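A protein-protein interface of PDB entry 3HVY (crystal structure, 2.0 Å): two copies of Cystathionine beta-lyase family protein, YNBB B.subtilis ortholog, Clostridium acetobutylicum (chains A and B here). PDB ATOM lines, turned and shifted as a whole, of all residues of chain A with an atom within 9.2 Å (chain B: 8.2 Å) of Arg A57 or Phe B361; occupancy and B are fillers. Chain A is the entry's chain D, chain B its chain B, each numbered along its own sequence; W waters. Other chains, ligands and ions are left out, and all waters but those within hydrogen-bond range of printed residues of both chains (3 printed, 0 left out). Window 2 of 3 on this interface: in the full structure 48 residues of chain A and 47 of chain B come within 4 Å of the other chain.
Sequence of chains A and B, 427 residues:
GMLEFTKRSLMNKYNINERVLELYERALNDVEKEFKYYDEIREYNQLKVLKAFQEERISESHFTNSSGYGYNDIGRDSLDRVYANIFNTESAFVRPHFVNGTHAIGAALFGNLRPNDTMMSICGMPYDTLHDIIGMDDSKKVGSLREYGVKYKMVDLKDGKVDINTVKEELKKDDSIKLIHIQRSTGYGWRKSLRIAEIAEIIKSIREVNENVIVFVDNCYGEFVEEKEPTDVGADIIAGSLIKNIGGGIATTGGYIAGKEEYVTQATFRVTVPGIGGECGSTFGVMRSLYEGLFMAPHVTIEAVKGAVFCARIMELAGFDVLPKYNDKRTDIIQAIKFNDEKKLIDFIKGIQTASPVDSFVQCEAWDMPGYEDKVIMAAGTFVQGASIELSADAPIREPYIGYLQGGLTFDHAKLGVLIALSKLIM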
ATOM      1  N   LEU A  50     -14.182 -33.678 -28.952  1.00  0.00           N
ATOM      2  CA  LEU A  50     -15.170 -33.423 -27.935  1.00  0.00           C
ATOM      3  C   LEU A  50     -14.483 -32.875 -26.674  1.00  0.00           C
ATOM      4  O   LEU A  50     -14.933 -31.881 -26.063  1.00  0.00           O
ATOM      5  CB  LEU A  50     -15.909 -34.725 -27.616  1.00  0.00           C
ATOM      6  CG  LEU A  50     -16.955 -34.670 -26.510  1.00  0.00           C
ATOM      7  CD1 LEU A  50     -18.034 -33.603 -26.862  1.00  0.00           C
ATOM      8  CD2 LEU A  50     -17.557 -36.074 -26.236  1.00  0.00           C
ATOM      9  N   LYS A  51     -13.398 -33.499 -26.247  1.00  0.00           N
ATOM     10  CA  LYS A  51     -12.715 -33.011 -25.035  1.00  0.00           C
ATOM     11  C   LYS A  51     -12.227 -31.566 -25.196  1.00  0.00           C
ATOM     12  O   LYS A  51     -12.277 -30.778 -24.269  1.00  0.00           O
ATOM     13  CB  LYS A  51     -11.494 -33.860 -24.691  1.00  0.00           C
ATOM     14  CG  LYS A  51     -11.765 -35.255 -24.200  1.00  0.00           C
ATOM     15  CD  LYS A  51     -10.519 -35.868 -23.541  1.00  0.00           C
ATOM     16  CE  LYS A  51      -9.266 -35.773 -24.395  1.00  0.00           C
ATOM     17  NZ  LYS A  51      -8.090 -36.466 -23.766  1.00  0.00           N
ATOM     18  N   ALA A  52     -11.672 -31.247 -26.361  1.00  0.00           N
ATOM     19  CA  ALA A  52     -11.179 -29.898 -26.646  1.00  0.00           C
ATOM     20  C   ALA A  52     -12.360 -28.865 -26.521  1.00  0.00           C
ATOM     21  O   ALA A  52     -12.228 -27.791 -25.887  1.00  0.00           O
ATOM     22  CB  ALA A  52     -10.518 -29.866 -28.017  1.00  0.00           C
ATOM     23  N   PHE A  53     -13.527 -29.200 -27.077  1.00  0.00           N
ATOM     24  CA  PHE A  53     -14.690 -28.332 -26.937  1.00  0.00           C
ATOM     25  C   PHE A  53     -15.023 -28.074 -25.452  1.00  0.00           C
ATOM     26  O   PHE A  53     -15.212 -26.940 -25.009  1.00  0.00           O
ATOM     27  CB  PHE A  53     -15.905 -28.977 -27.613  1.00  0.00           C
ATOM     28  CG  PHE A  53     -16.106 -28.579 -29.082  1.00  0.00           C
ATOM     29  CD1 PHE A  53     -15.325 -29.118 -30.090  1.00  0.00           C
ATOM     30  CD2 PHE A  53     -17.116 -27.703 -29.436  1.00  0.00           C
ATOM     31  CE1 PHE A  53     -15.525 -28.770 -31.409  1.00  0.00           C
ATOM     32  CE2 PHE A  53     -17.342 -27.338 -30.757  1.00  0.00           C
ATOM     33  CZ  PHE A  53     -16.533 -27.858 -31.751  1.00  0.00           C
ATOM     34  N   GLN A  54     -15.079 -29.160 -24.702  1.00  0.00           N
ATOM     35  CA  GLN A  54     -15.479 -29.126 -23.291  1.00  0.00           C
ATOM     36  C   GLN A  54     -14.445 -28.447 -22.438  1.00  0.00           C
ATOM     37  O   GLN A  54     -14.808 -27.688 -21.556  1.00  0.00           O
ATOM     38  CB  GLN A  54     -15.751 -30.554 -22.827  1.00  0.00           C
ATOM     39  CG  GLN A  54     -16.866 -31.211 -23.665  1.00  0.00           C
ATOM     40  CD  GLN A  54     -17.330 -32.504 -23.048  1.00  0.00           C
ATOM     41  OE1 GLN A  54     -16.540 -33.185 -22.391  1.00  0.00           O
ATOM     42  NE2 GLN A  54     -18.598 -32.854 -23.248  1.00  0.00           N
ATOM     43  N   GLU A  55     -13.156 -28.607 -22.755  1.00  0.00           N
ATOM     44  CA  GLU A  55     -12.128 -27.914 -21.987  1.00  0.00           C
ATOM     45  C   GLU A  55     -12.123 -26.405 -22.261  1.00  0.00           C
ATOM     46  O   GLU A  55     -11.775 -25.637 -21.396  1.00  0.00           O
ATOM     47  CB  GLU A  55     -10.757 -28.552 -22.182  1.00  0.00           C
ATOM     48  CG  GLU A  55     -10.724 -29.996 -21.558  1.00  0.00           C
ATOM     49  CD  GLU A  55      -9.539 -30.878 -21.971  1.00  0.00           C
ATOM     50  OE1 GLU A  55      -8.648 -30.426 -22.731  1.00  0.00           O
ATOM     51  OE2 GLU A  55      -9.519 -32.046 -21.516  1.00  0.00           O
ATOM     52  N   GLU A  56     -12.586 -25.979 -23.419  1.00  0.00           N
ATOM     53  CA  GLU A  56     -12.698 -24.561 -23.688  1.00  0.00           C
ATOM     54  C   GLU A  56     -14.082 -24.008 -23.309  1.00  0.00           C
ATOM     55  O   GLU A  56     -14.361 -22.835 -23.501  1.00  0.00           O
ATOM     56  CB  GLU A  56     -12.332 -24.272 -25.156  1.00  0.00           C
ATOM     57  CG  GLU A  56     -12.342 -22.779 -25.597  1.00  0.00           C
ATOM     58  CD  GLU A  56     -11.353 -21.877 -24.844  1.00  0.00           C
ATOM     59  OE1 GLU A  56     -10.363 -22.409 -24.271  1.00  0.00           O
ATOM     60  OE2 GLU A  56     -11.562 -20.630 -24.865  1.00  0.00           O
ATOM     61  N   ARG A  57     -14.937 -24.838 -22.728  1.00  0.00           N
ATOM     62  CA  ARG A  57     -16.276 -24.446 -22.355  1.00  0.00           C
ATOM     63  C   ARG A  57     -17.060 -23.753 -23.491  1.00  0.00           C
ATOM     64  O   ARG A  57     -17.674 -22.698 -23.326  1.00  0.00           O
ATOM     65  CB  ARG A  57     -16.261 -23.599 -21.082  1.00  0.00           C
ATOM     66  CG  ARG A  57     -15.657 -24.280 -19.887  1.00  0.00           C
ATOM     67  CD  ARG A  57     -15.686 -23.370 -18.673  1.00  0.00           C
ATOM     68  NE  ARG A  57     -15.895 -24.198 -17.489  1.00  0.00           N
ATOM     69  CZ  ARG A  57     -17.002 -24.231 -16.739  1.00  0.00           C
ATOM     70  NH1 ARG A  57     -18.045 -23.433 -16.967  1.00  0.00           N
ATOM     71  NH2 ARG A  57     -17.041 -25.059 -15.705  1.00  0.00           N
ATOM     72  N   ILE A  58     -17.061 -24.374 -24.651  1.00  0.00           N
ATOM     73  CA  ILE A  58     -17.784 -23.824 -25.756  1.00  0.00           C
ATOM     74  C   ILE A  58     -19.259 -23.764 -25.408  1.00  0.00           C
ATOM     75  O   ILE A  58     -19.796 -24.705 -24.809  1.00  0.00           O
ATOM     76  CB  ILE A  58     -17.480 -24.604 -27.051  1.00  0.00           C
ATOM     77  CG1 ILE A  58     -15.979 -24.459 -27.380  1.00  0.00           C
ATOM     78  CG2 ILE A  58     -18.360 -24.141 -28.189  1.00  0.00           C
ATOM     79  CD1 ILE A  58     -15.450 -23.020 -27.518  1.00  0.00           C
ATOM     80  N   SER A  59     -19.884 -22.618 -25.713  1.00  0.00           N
ATOM     81  CA  SER A  59     -21.306 -22.412 -25.523  1.00  0.00           C
ATOM     82  C   SER A  59     -21.904 -21.657 -26.693  1.00  0.00           C
ATOM     83  O   SER A  59     -21.182 -21.216 -27.635  1.00  0.00           O
ATOM     84  CB  SER A  59     -21.572 -21.627 -24.243  1.00  0.00           C
ATOM     85  OG  SER A  59     -21.003 -20.375 -24.386  1.00  0.00           O
ATOM     86  N   GLU A  60     -23.220 -21.461 -26.627  1.00  0.00           N
ATOM     87  CA  GLU A  60     -23.937 -20.686 -27.670  1.00  0.00           C
ATOM     88  C   GLU A  60     -23.310 -19.282 -27.848  1.00  0.00           C
ATOM     89  O   GLU A  60     -23.230 -18.780 -28.964  1.00  0.00           O
ATOM     90  CB  GLU A  60     -25.453 -20.629 -27.404  1.00  0.00           C
ATOM     91  N   SER A  61     -22.782 -18.698 -26.771  1.00  0.00           N
ATOM     92  CA  SER A  61     -22.186 -17.364 -26.867  1.00  0.00           C
ATOM     93  C   SER A  61     -20.882 -17.284 -27.695  1.00  0.00           C
ATOM     94  O   SER A  61     -20.393 -16.197 -28.048  1.00  0.00           O
ATOM     95  CB  SER A  61     -21.991 -16.777 -25.485  1.00  0.00           C
ATOM     96  OG  SER A  61     -21.367 -17.688 -24.624  1.00  0.00           O
ATOM     97  N   HIS A  62     -20.320 -18.439 -28.017  1.00  0.00           N
ATOM     98  CA  HIS A  62     -19.186 -18.503 -28.948  1.00  0.00           C
ATOM     99  C   HIS A  62     -19.631 -18.428 -30.391  1.00  0.00           C
ATOM    100  O   HIS A  62     -18.768 -18.307 -31.296  1.00  0.00           O
ATOM    101  CB  HIS A  62     -18.380 -19.783 -28.702  1.00  0.00           C
ATOM    102  CG  HIS A  62     -17.655 -19.746 -27.405  1.00  0.00           C
ATOM    103  ND1 HIS A  62     -18.183 -20.278 -26.238  1.00  0.00           N
ATOM    104  CD2 HIS A  62     -16.496 -19.150 -27.058  1.00  0.00           C
ATOM    105  CE1 HIS A  62     -17.344 -20.054 -25.244  1.00  0.00           C
ATOM    106  NE2 HIS A  62     -16.325 -19.353 -25.710  1.00  0.00           N
ATOM    107  N   PHE A  63     -20.950 -18.506 -30.631  1.00  0.00           N
ATOM    108  CA  PHE A  63     -21.470 -18.422 -32.022  1.00  0.00           C
ATOM    109  C   PHE A  63     -21.759 -16.932 -32.327  1.00  0.00           C
ATOM    110  O   PHE A  63     -22.894 -16.465 -32.444  1.00  0.00           O
ATOM    111  CB  PHE A  63     -22.676 -19.342 -32.285  1.00  0.00           C
ATOM    112  CG  PHE A  63     -22.463 -20.795 -31.840  1.00  0.00           C
ATOM    113  CD1 PHE A  63     -21.207 -21.384 -31.929  1.00  0.00           C
ATOM    114  CD2 PHE A  63     -23.523 -21.564 -31.397  1.00  0.00           C
ATOM    115  CE1 PHE A  63     -20.995 -22.683 -31.534  1.00  0.00           C
ATOM    116  CE2 PHE A  63     -23.306 -22.897 -30.995  1.00  0.00           C
ATOM    117  CZ  PHE A  63     -22.018 -23.429 -31.088  1.00  0.00           C
ATOM    118  N   ILE A  74     -15.073 -13.462 -29.108  1.00  0.00           N
ATOM    119  CA  ILE A  74     -14.777 -14.602 -28.240  1.00  0.00           C
ATOM    120  C   ILE A  74     -14.917 -15.934 -28.956  1.00  0.00           C
ATOM    121  O   ILE A  74     -14.201 -16.876 -28.623  1.00  0.00           O
ATOM    122  CB  ILE A  74     -15.598 -14.589 -26.896  1.00  0.00           C
ATOM    123  CG1 ILE A  74     -17.080 -14.984 -27.124  1.00  0.00           C
ATOM    124  CG2 ILE A  74     -15.445 -13.232 -26.212  1.00  0.00           C
ATOM    125  CD1 ILE A  74     -17.868 -15.135 -25.878  1.00  0.00           C
ATOM    126  N   SER A  78     -11.746 -18.391 -29.090  1.00  0.00           N
ATOM    127  CA  SER A  78     -11.885 -19.702 -28.487  1.00  0.00           C
ATOM    128  C   SER A  78     -11.699 -20.816 -29.507  1.00  0.00           C
ATOM    129  O   SER A  78     -11.247 -21.940 -29.146  1.00  0.00           O
ATOM    130  CB  SER A  78     -13.264 -19.829 -27.829  1.00  0.00           C
ATOM    131  OG  SER A  78     -13.370 -19.050 -26.641  1.00  0.00           O
ATOM    132  N   ARG A  81      -8.173 -21.539 -29.557  1.00  0.00           N
ATOM    133  CA  ARG A  81      -7.754 -22.345 -28.410  1.00  0.00           C
ATOM    134  C   ARG A  81      -8.152 -23.812 -28.575  1.00  0.00           C
ATOM    135  O   ARG A  81      -7.382 -24.718 -28.241  1.00  0.00           O
ATOM    136  CB  ARG A  81      -8.305 -21.782 -27.123  1.00  0.00           C
ATOM    137  CG  ARG A  81      -7.598 -20.502 -26.724  1.00  0.00           C
ATOM    138  CD  ARG A  81      -7.959 -20.065 -25.302  1.00  0.00           C
ATOM    139  NE  ARG A  81      -9.273 -19.433 -25.262  1.00  0.00           N
ATOM    140  CZ  ARG A  81      -9.507 -18.146 -25.558  1.00  0.00           C
ATOM    141  NH1 ARG A  81      -8.531 -17.297 -25.851  1.00  0.00           N
ATOM    142  NH2 ARG A  81     -10.737 -17.685 -25.513  1.00  0.00           N
ATOM    143  N   VAL A  82      -9.326 -24.059 -29.155  1.00  0.00           N
ATOM    144  CA  VAL A  82      -9.780 -25.451 -29.381  1.00  0.00           C
ATOM    145  C   VAL A  82      -8.821 -26.181 -30.357  1.00  0.00           C
ATOM    146  O   VAL A  82      -8.385 -27.299 -30.081  1.00  0.00           O
ATOM    147  CB  VAL A  82     -11.266 -25.486 -29.856  1.00  0.00           C
ATOM    148  CG1 VAL A  82     -11.646 -26.872 -30.390  1.00  0.00           C
ATOM    149  CG2 VAL A  82     -12.214 -25.033 -28.661  1.00  0.00           C
ATOM    150  N   ASN A  85      -5.475 -26.947 -28.753  1.00  0.00           N
ATOM    151  CA  ASN A  85      -5.639 -28.119 -27.884  1.00  0.00           C
ATOM    152  C   ASN A  85      -5.633 -29.423 -28.715  1.00  0.00           C
ATOM    153  O   ASN A  85      -4.897 -30.382 -28.413  1.00  0.00           O
ATOM    154  CB  ASN A  85      -6.949 -28.002 -27.141  1.00  0.00           C
ATOM    155  CG  ASN A  85      -7.043 -28.944 -25.945  1.00  0.00           C
ATOM    156  OD1 ASN A  85      -6.181 -29.818 -25.739  1.00  0.00           O
ATOM    157  ND2 ASN A  85      -8.066 -28.738 -25.115  1.00  0.00           N
ATOM    158  N   TYR A 291     -17.232 -24.322 -35.952  1.00  0.00           N
ATOM    159  CA  TYR A 291     -17.248 -25.216 -34.804  1.00  0.00           C
ATOM    160  C   TYR A 291     -17.943 -26.523 -35.140  1.00  0.00           C
ATOM    161  O   TYR A 291     -17.443 -27.590 -34.842  1.00  0.00           O
ATOM    162  CB  TYR A 291     -18.003 -24.579 -33.599  1.00  0.00           C
ATOM    163  CG  TYR A 291     -17.204 -23.566 -32.754  1.00  0.00           C
ATOM    164  CD1 TYR A 291     -16.296 -24.004 -31.788  1.00  0.00           C
ATOM    165  CD2 TYR A 291     -17.397 -22.202 -32.886  1.00  0.00           C
ATOM    166  CE1 TYR A 291     -15.612 -23.118 -31.002  1.00  0.00           C
ATOM    167  CE2 TYR A 291     -16.705 -21.309 -32.119  1.00  0.00           C
ATOM    168  CZ  TYR A 291     -15.808 -21.764 -31.172  1.00  0.00           C
ATOM    169  OH  TYR A 291     -15.071 -20.887 -30.392  1.00  0.00           O
ATOM    170  N   GLN B 353     -25.919 -34.461 -21.038  1.00  0.00           N
ATOM    171  CA  GLN B 353     -25.477 -33.070 -21.130  1.00  0.00           C
ATOM    172  C   GLN B 353     -23.936 -33.010 -20.968  1.00  0.00           C
ATOM    173  O   GLN B 353     -23.268 -32.294 -21.703  1.00  0.00           O
ATOM    174  CB  GLN B 353     -26.179 -32.159 -20.111  1.00  0.00           C
ATOM    175  CG  GLN B 353     -25.819 -30.647 -20.217  1.00  0.00           C
ATOM    176  CD  GLN B 353     -26.527 -29.900 -21.359  1.00  0.00           C
ATOM    177  OE1 GLN B 353     -27.680 -30.193 -21.673  1.00  0.00           O
ATOM    178  NE2 GLN B 353     -25.849 -28.899 -21.941  1.00  0.00           N
ATOM    179  N   THR B 354     -23.347 -33.773 -20.051  1.00  0.00           N
ATOM    180  CA  THR B 354     -21.892 -33.652 -19.881  1.00  0.00           C
ATOM    181  C   THR B 354     -21.140 -34.231 -21.087  1.00  0.00           C
ATOM    182  O   THR B 354     -19.962 -33.951 -21.276  1.00  0.00           O
ATOM    183  CB  THR B 354     -21.401 -34.324 -18.595  1.00  0.00           C
ATOM    184  OG1 THR B 354     -21.562 -35.744 -18.704  1.00  0.00           O
ATOM    185  CG2 THR B 354     -22.209 -33.829 -17.402  1.00  0.00           C
ATOM    186  N   ALA B 355     -21.817 -35.062 -21.877  1.00  0.00           N
ATOM    187  CA  ALA B 355     -21.231 -35.639 -23.089  1.00  0.00           C
ATOM    188  C   ALA B 355     -21.381 -34.706 -24.277  1.00  0.00           C
ATOM    189  O   ALA B 355     -20.972 -35.062 -25.375  1.00  0.00           O
ATOM    190  CB  ALA B 355     -21.945 -36.941 -23.419  1.00  0.00           C
ATOM    191  N   SER B 356     -21.998 -33.526 -24.095  1.00  0.00           N
ATOM    192  CA  SER B 356     -22.310 -32.684 -25.239  1.00  0.00           C
ATOM    193  C   SER B 356     -21.182 -31.723 -25.572  1.00  0.00           C
ATOM    194  O   SER B 356     -20.455 -31.305 -24.680  1.00  0.00           O
ATOM    195  CB  SER B 356     -23.642 -31.930 -25.012  1.00  0.00           C
ATOM    196  OG  SER B 356     -24.707 -32.868 -24.836  1.00  0.00           O
ATOM    197  N   PRO B 357     -21.001 -31.390 -26.879  1.00  0.00           N
ATOM    198  CA  PRO B 357     -19.934 -30.454 -27.235  1.00  0.00           C
ATOM    199  C   PRO B 357     -20.198 -28.976 -26.850  1.00  0.00           C
ATOM    200  O   PRO B 357     -19.250 -28.232 -26.616  1.00  0.00           O
ATOM    201  CB  PRO B 357     -19.827 -30.624 -28.778  1.00  0.00           C
ATOM    202  CG  PRO B 357     -21.172 -30.985 -29.219  1.00  0.00           C
ATOM    203  CD  PRO B 357     -21.732 -31.856 -28.072  1.00  0.00           C
ATOM    204  N   VAL B 358     -21.465 -28.560 -26.824  1.00  0.00           N
ATOM    205  CA  VAL B 358     -21.843 -27.177 -26.518  1.00  0.00           C
ATOM    206  C   VAL B 358     -22.561 -27.131 -25.200  1.00  0.00           C
ATOM    207  O   VAL B 358     -23.419 -27.980 -24.907  1.00  0.00           O
ATOM    208  CB  VAL B 358     -22.743 -26.596 -27.641  1.00  0.00           C
ATOM    209  CG1 VAL B 358     -23.040 -25.101 -27.428  1.00  0.00           C
ATOM    210  CG2 VAL B 358     -22.043 -26.771 -28.981  1.00  0.00           C
ATOM    211  N   ASP B 359     -22.179 -26.177 -24.355  1.00  0.00           N
ATOM    212  CA  ASP B 359     -22.815 -26.041 -23.042  1.00  0.00           C
ATOM    213  C   ASP B 359     -22.740 -27.325 -22.180  1.00  0.00           C
ATOM    214  O   ASP B 359     -23.638 -27.601 -21.362  1.00  0.00           O
ATOM    215  CB  ASP B 359     -24.262 -25.529 -23.230  1.00  0.00           C
ATOM    216  CG  ASP B 359     -24.298 -24.032 -23.663  1.00  0.00           C
ATOM    217  OD1 ASP B 359     -23.531 -23.256 -23.100  1.00  0.00           O
ATOM    218  OD2 ASP B 359     -25.073 -23.652 -24.553  1.00  0.00           O
ATOM    219  N   SER B 360     -21.627 -28.070 -22.326  1.00  0.00           N
ATOM    220  CA  SER B 360     -21.397 -29.309 -21.565  1.00  0.00           C
ATOM    221  C   SER B 360     -21.368 -29.060 -20.046  1.00  0.00           C
ATOM    222  O   SER B 360     -21.616 -29.977 -19.244  1.00  0.00           O
ATOM    223  CB  SER B 360     -20.064 -29.912 -21.978  1.00  0.00           C
ATOM    224  OG  SER B 360     -18.978 -28.996 -21.760  1.00  0.00           O
ATOM    225  N   PHE B 361     -21.025 -27.830 -19.656  1.00  0.00           N
ATOM    226  CA  PHE B 361     -20.905 -27.435 -18.235  1.00  0.00           C
ATOM    227  C   PHE B 361     -22.218 -26.925 -17.622  1.00  0.00           C
ATOM    228  O   PHE B 361     -22.271 -26.666 -16.438  1.00  0.00           O
ATOM    229  CB  PHE B 361     -19.856 -26.304 -18.122  1.00  0.00           C
ATOM    230  CG  PHE B 361     -20.200 -25.098 -18.966  1.00  0.00           C
ATOM    231  CD1 PHE B 361     -21.035 -24.091 -18.464  1.00  0.00           C
ATOM    232  CD2 PHE B 361     -19.748 -25.003 -20.285  1.00  0.00           C
ATOM    233  CE1 PHE B 361     -21.380 -22.991 -19.261  1.00  0.00           C
ATOM    234  CE2 PHE B 361     -20.090 -23.924 -21.090  1.00  0.00           C
ATOM    235  CZ  PHE B 361     -20.893 -22.910 -20.580  1.00  0.00           C
ATOM    236  N   VAL B 362     -23.246 -26.728 -18.427  1.00  0.00           N
ATOM    237  CA  VAL B 362     -24.499 -26.145 -17.968  1.00  0.00           C
ATOM    238  C   VAL B 362     -25.313 -27.168 -17.170  1.00  0.00           C
ATOM    239  O   VAL B 362     -25.478 -28.327 -17.585  1.00  0.00           O
ATOM    240  CB  VAL B 362     -25.311 -25.576 -19.160  1.00  0.00           C
ATOM    241  CG1 VAL B 362     -26.682 -25.150 -18.732  1.00  0.00           C
ATOM    242  CG2 VAL B 362     -24.550 -24.392 -19.819  1.00  0.00           C
ATOM    243  N   GLN B 363     -25.800 -26.730 -16.008  1.00  0.00           N
ATOM    244  CA  GLN B 363     -26.584 -27.587 -15.110  1.00  0.00           C
ATOM    245  C   GLN B 363     -27.979 -27.828 -15.710  1.00  0.00           C
ATOM    246  O   GLN B 363     -28.522 -26.970 -16.440  1.00  0.00           O
ATOM    247  CB  GLN B 363     -26.677 -26.952 -13.705  1.00  0.00           C
ATOM    248  N   CYS B 364     -28.528 -29.017 -15.459  1.00  0.00           N
ATOM    249  CA  CYS B 364     -29.910 -29.317 -15.868  1.00  0.00           C
ATOM    250  C   CYS B 364     -30.609 -30.227 -14.865  1.00  0.00           C
ATOM    251  O   CYS B 364     -31.213 -29.727 -13.909  1.00  0.00           O
ATOM    252  CB  CYS B 364     -29.996 -29.841 -17.320  1.00  0.00           C
ATOM    253  SG  CYS B 364     -29.162 -31.408 -17.745  1.00  0.00           S
ATOM    254  N   GLY B 381     -27.224 -29.786 -25.448  1.00  0.00           N
ATOM    255  CA  GLY B 381     -25.984 -29.059 -25.701  1.00  0.00           C
ATOM    256  C   GLY B 381     -25.610 -29.228 -27.150  1.00  0.00           C
ATOM    257  O   GLY B 381     -24.733 -30.043 -27.498  1.00  0.00           O
HETATM  258  O   HOH W   1     -17.168 -27.770 -19.994  1.00  0.00           O
HETATM  259  O   HOH W   2     -18.224 -32.143 -19.645  1.00  0.00           O
HETATM  260  O   HOH W   3     -18.984 -27.285 -23.970  1.00  0.00           O
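Water W3 lies within hydrogen-bond range of the side-chain hydroxyl of Ser B360 (2.8 Å), the backbone carbonyl oxygen of Pro B357 (2.8 Å), the backbone carbonyl oxygen of Ile A58 (2.8 Å) and the backbone NH of Asp B359 (3.4 Å). Water W1 bridges the side-chain hydroxyl (OG) of Ser B360 (2.8 Å) and the backbone carbonyl oxygen (O) of Gln A54 (2.8 Å). Water W2 lies within hydrogen-bond range of O of Thr B354 (3.0 Å) and OE1 of Gln A54 (3.4 Å).
Leu A50 touches Pro B357. O of Pro B357 touches CB of Phe A53, at 3.6 Å. Gln A54 touches Ser B360. Phe B361 touches Arg A57. Val B358 touches Ile A58. Val B358 touches Ser A59 (CG1 to C, 3.7 Å). Ser A59 touches Phe B361. Glu A60 touches Val B358. N of Glu A60 touches OD2 of Asp B359, at 3.5 Å. Phe A63 touches Val B358 (CZ to CG2, 3.95 Å).
Of the printed residues of chain B, Phe A53 touches Pro B357. Glu A55 touches none of the printed residues of chain B. Of chain B, only Phe B361 comes within 4 Å of Arg A57. Of the printed residues of chain A, Pro B357 touches Leu A50 and Phe A53. Of chain A, only Arg A57 (3.4 Å), Ile A58 (3.8 Å) and Ser A59 (3.9 Å) come within 4 Å of Phe B361. No residue of chain A comes within 4 Å of Val B362. The nearest residue of chain B that does not touch Arg A57 is Ser B360 (5.3 Å). The nearest residue of chain A that does not touch Phe B361 is Gln A54 (5.8 Å). The nearest printed residue of chain B that does not touch Phe A63 is Asp B359 (6.7 Å).
The backbone carbonyl oxygen (O) of Thr B354 is in hydrogen-bond range of the side-chain amide nitrogen (NE2) of Gln A54, 2.6 Å away. O of Ser B356 sits at hydrogen-bond distance from NE2 of Gln A54, 2.8 Å away. O of Ile A58 is in hydrogen-bond range of N of Asp B359.
No position is printed for both chains.
Of the 20 printed residues of chain A, 8 touch a printed residue of chain B. Printed residues of chain A that touch a printed residue of chain B: Leu A50, Phe A53, Gln A54, Arg A57, Ile A58, Ser A59, Glu A60 and Phe A63. Hydrophobic or aromatic side chains of chain A that line the printed part of chain B: Leu A50, Phe A53 and Phe A63. Along chain B the printed residues that touch a printed residue of chain A span positions 354 to 361. Among the printed residues, no Asp or Glu carboxylate lies within 4 Å of a Lys or Arg side-chain nitrogen of the other chain.
O of Gln B353 lies close to OG of Ser B356 (3.5 Å). NE2 of Gln B353 lies within hydrogen-bond range of O of Asp B359, at 2.6 Å. N of Ile A58 sits at hydrogen-bond distance from O of Phe A53, at 3.2 Å. The side-chain hydroxyl (OG) of Ser A59 lies within hydrogen-bond range of the side-chain hydroxyl (OG) of Ser A61 (2.7 Å). The backbone NH of Ser A59 sits at hydrogen-bond distance from a ring nitrogen (ND1) of His A62.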
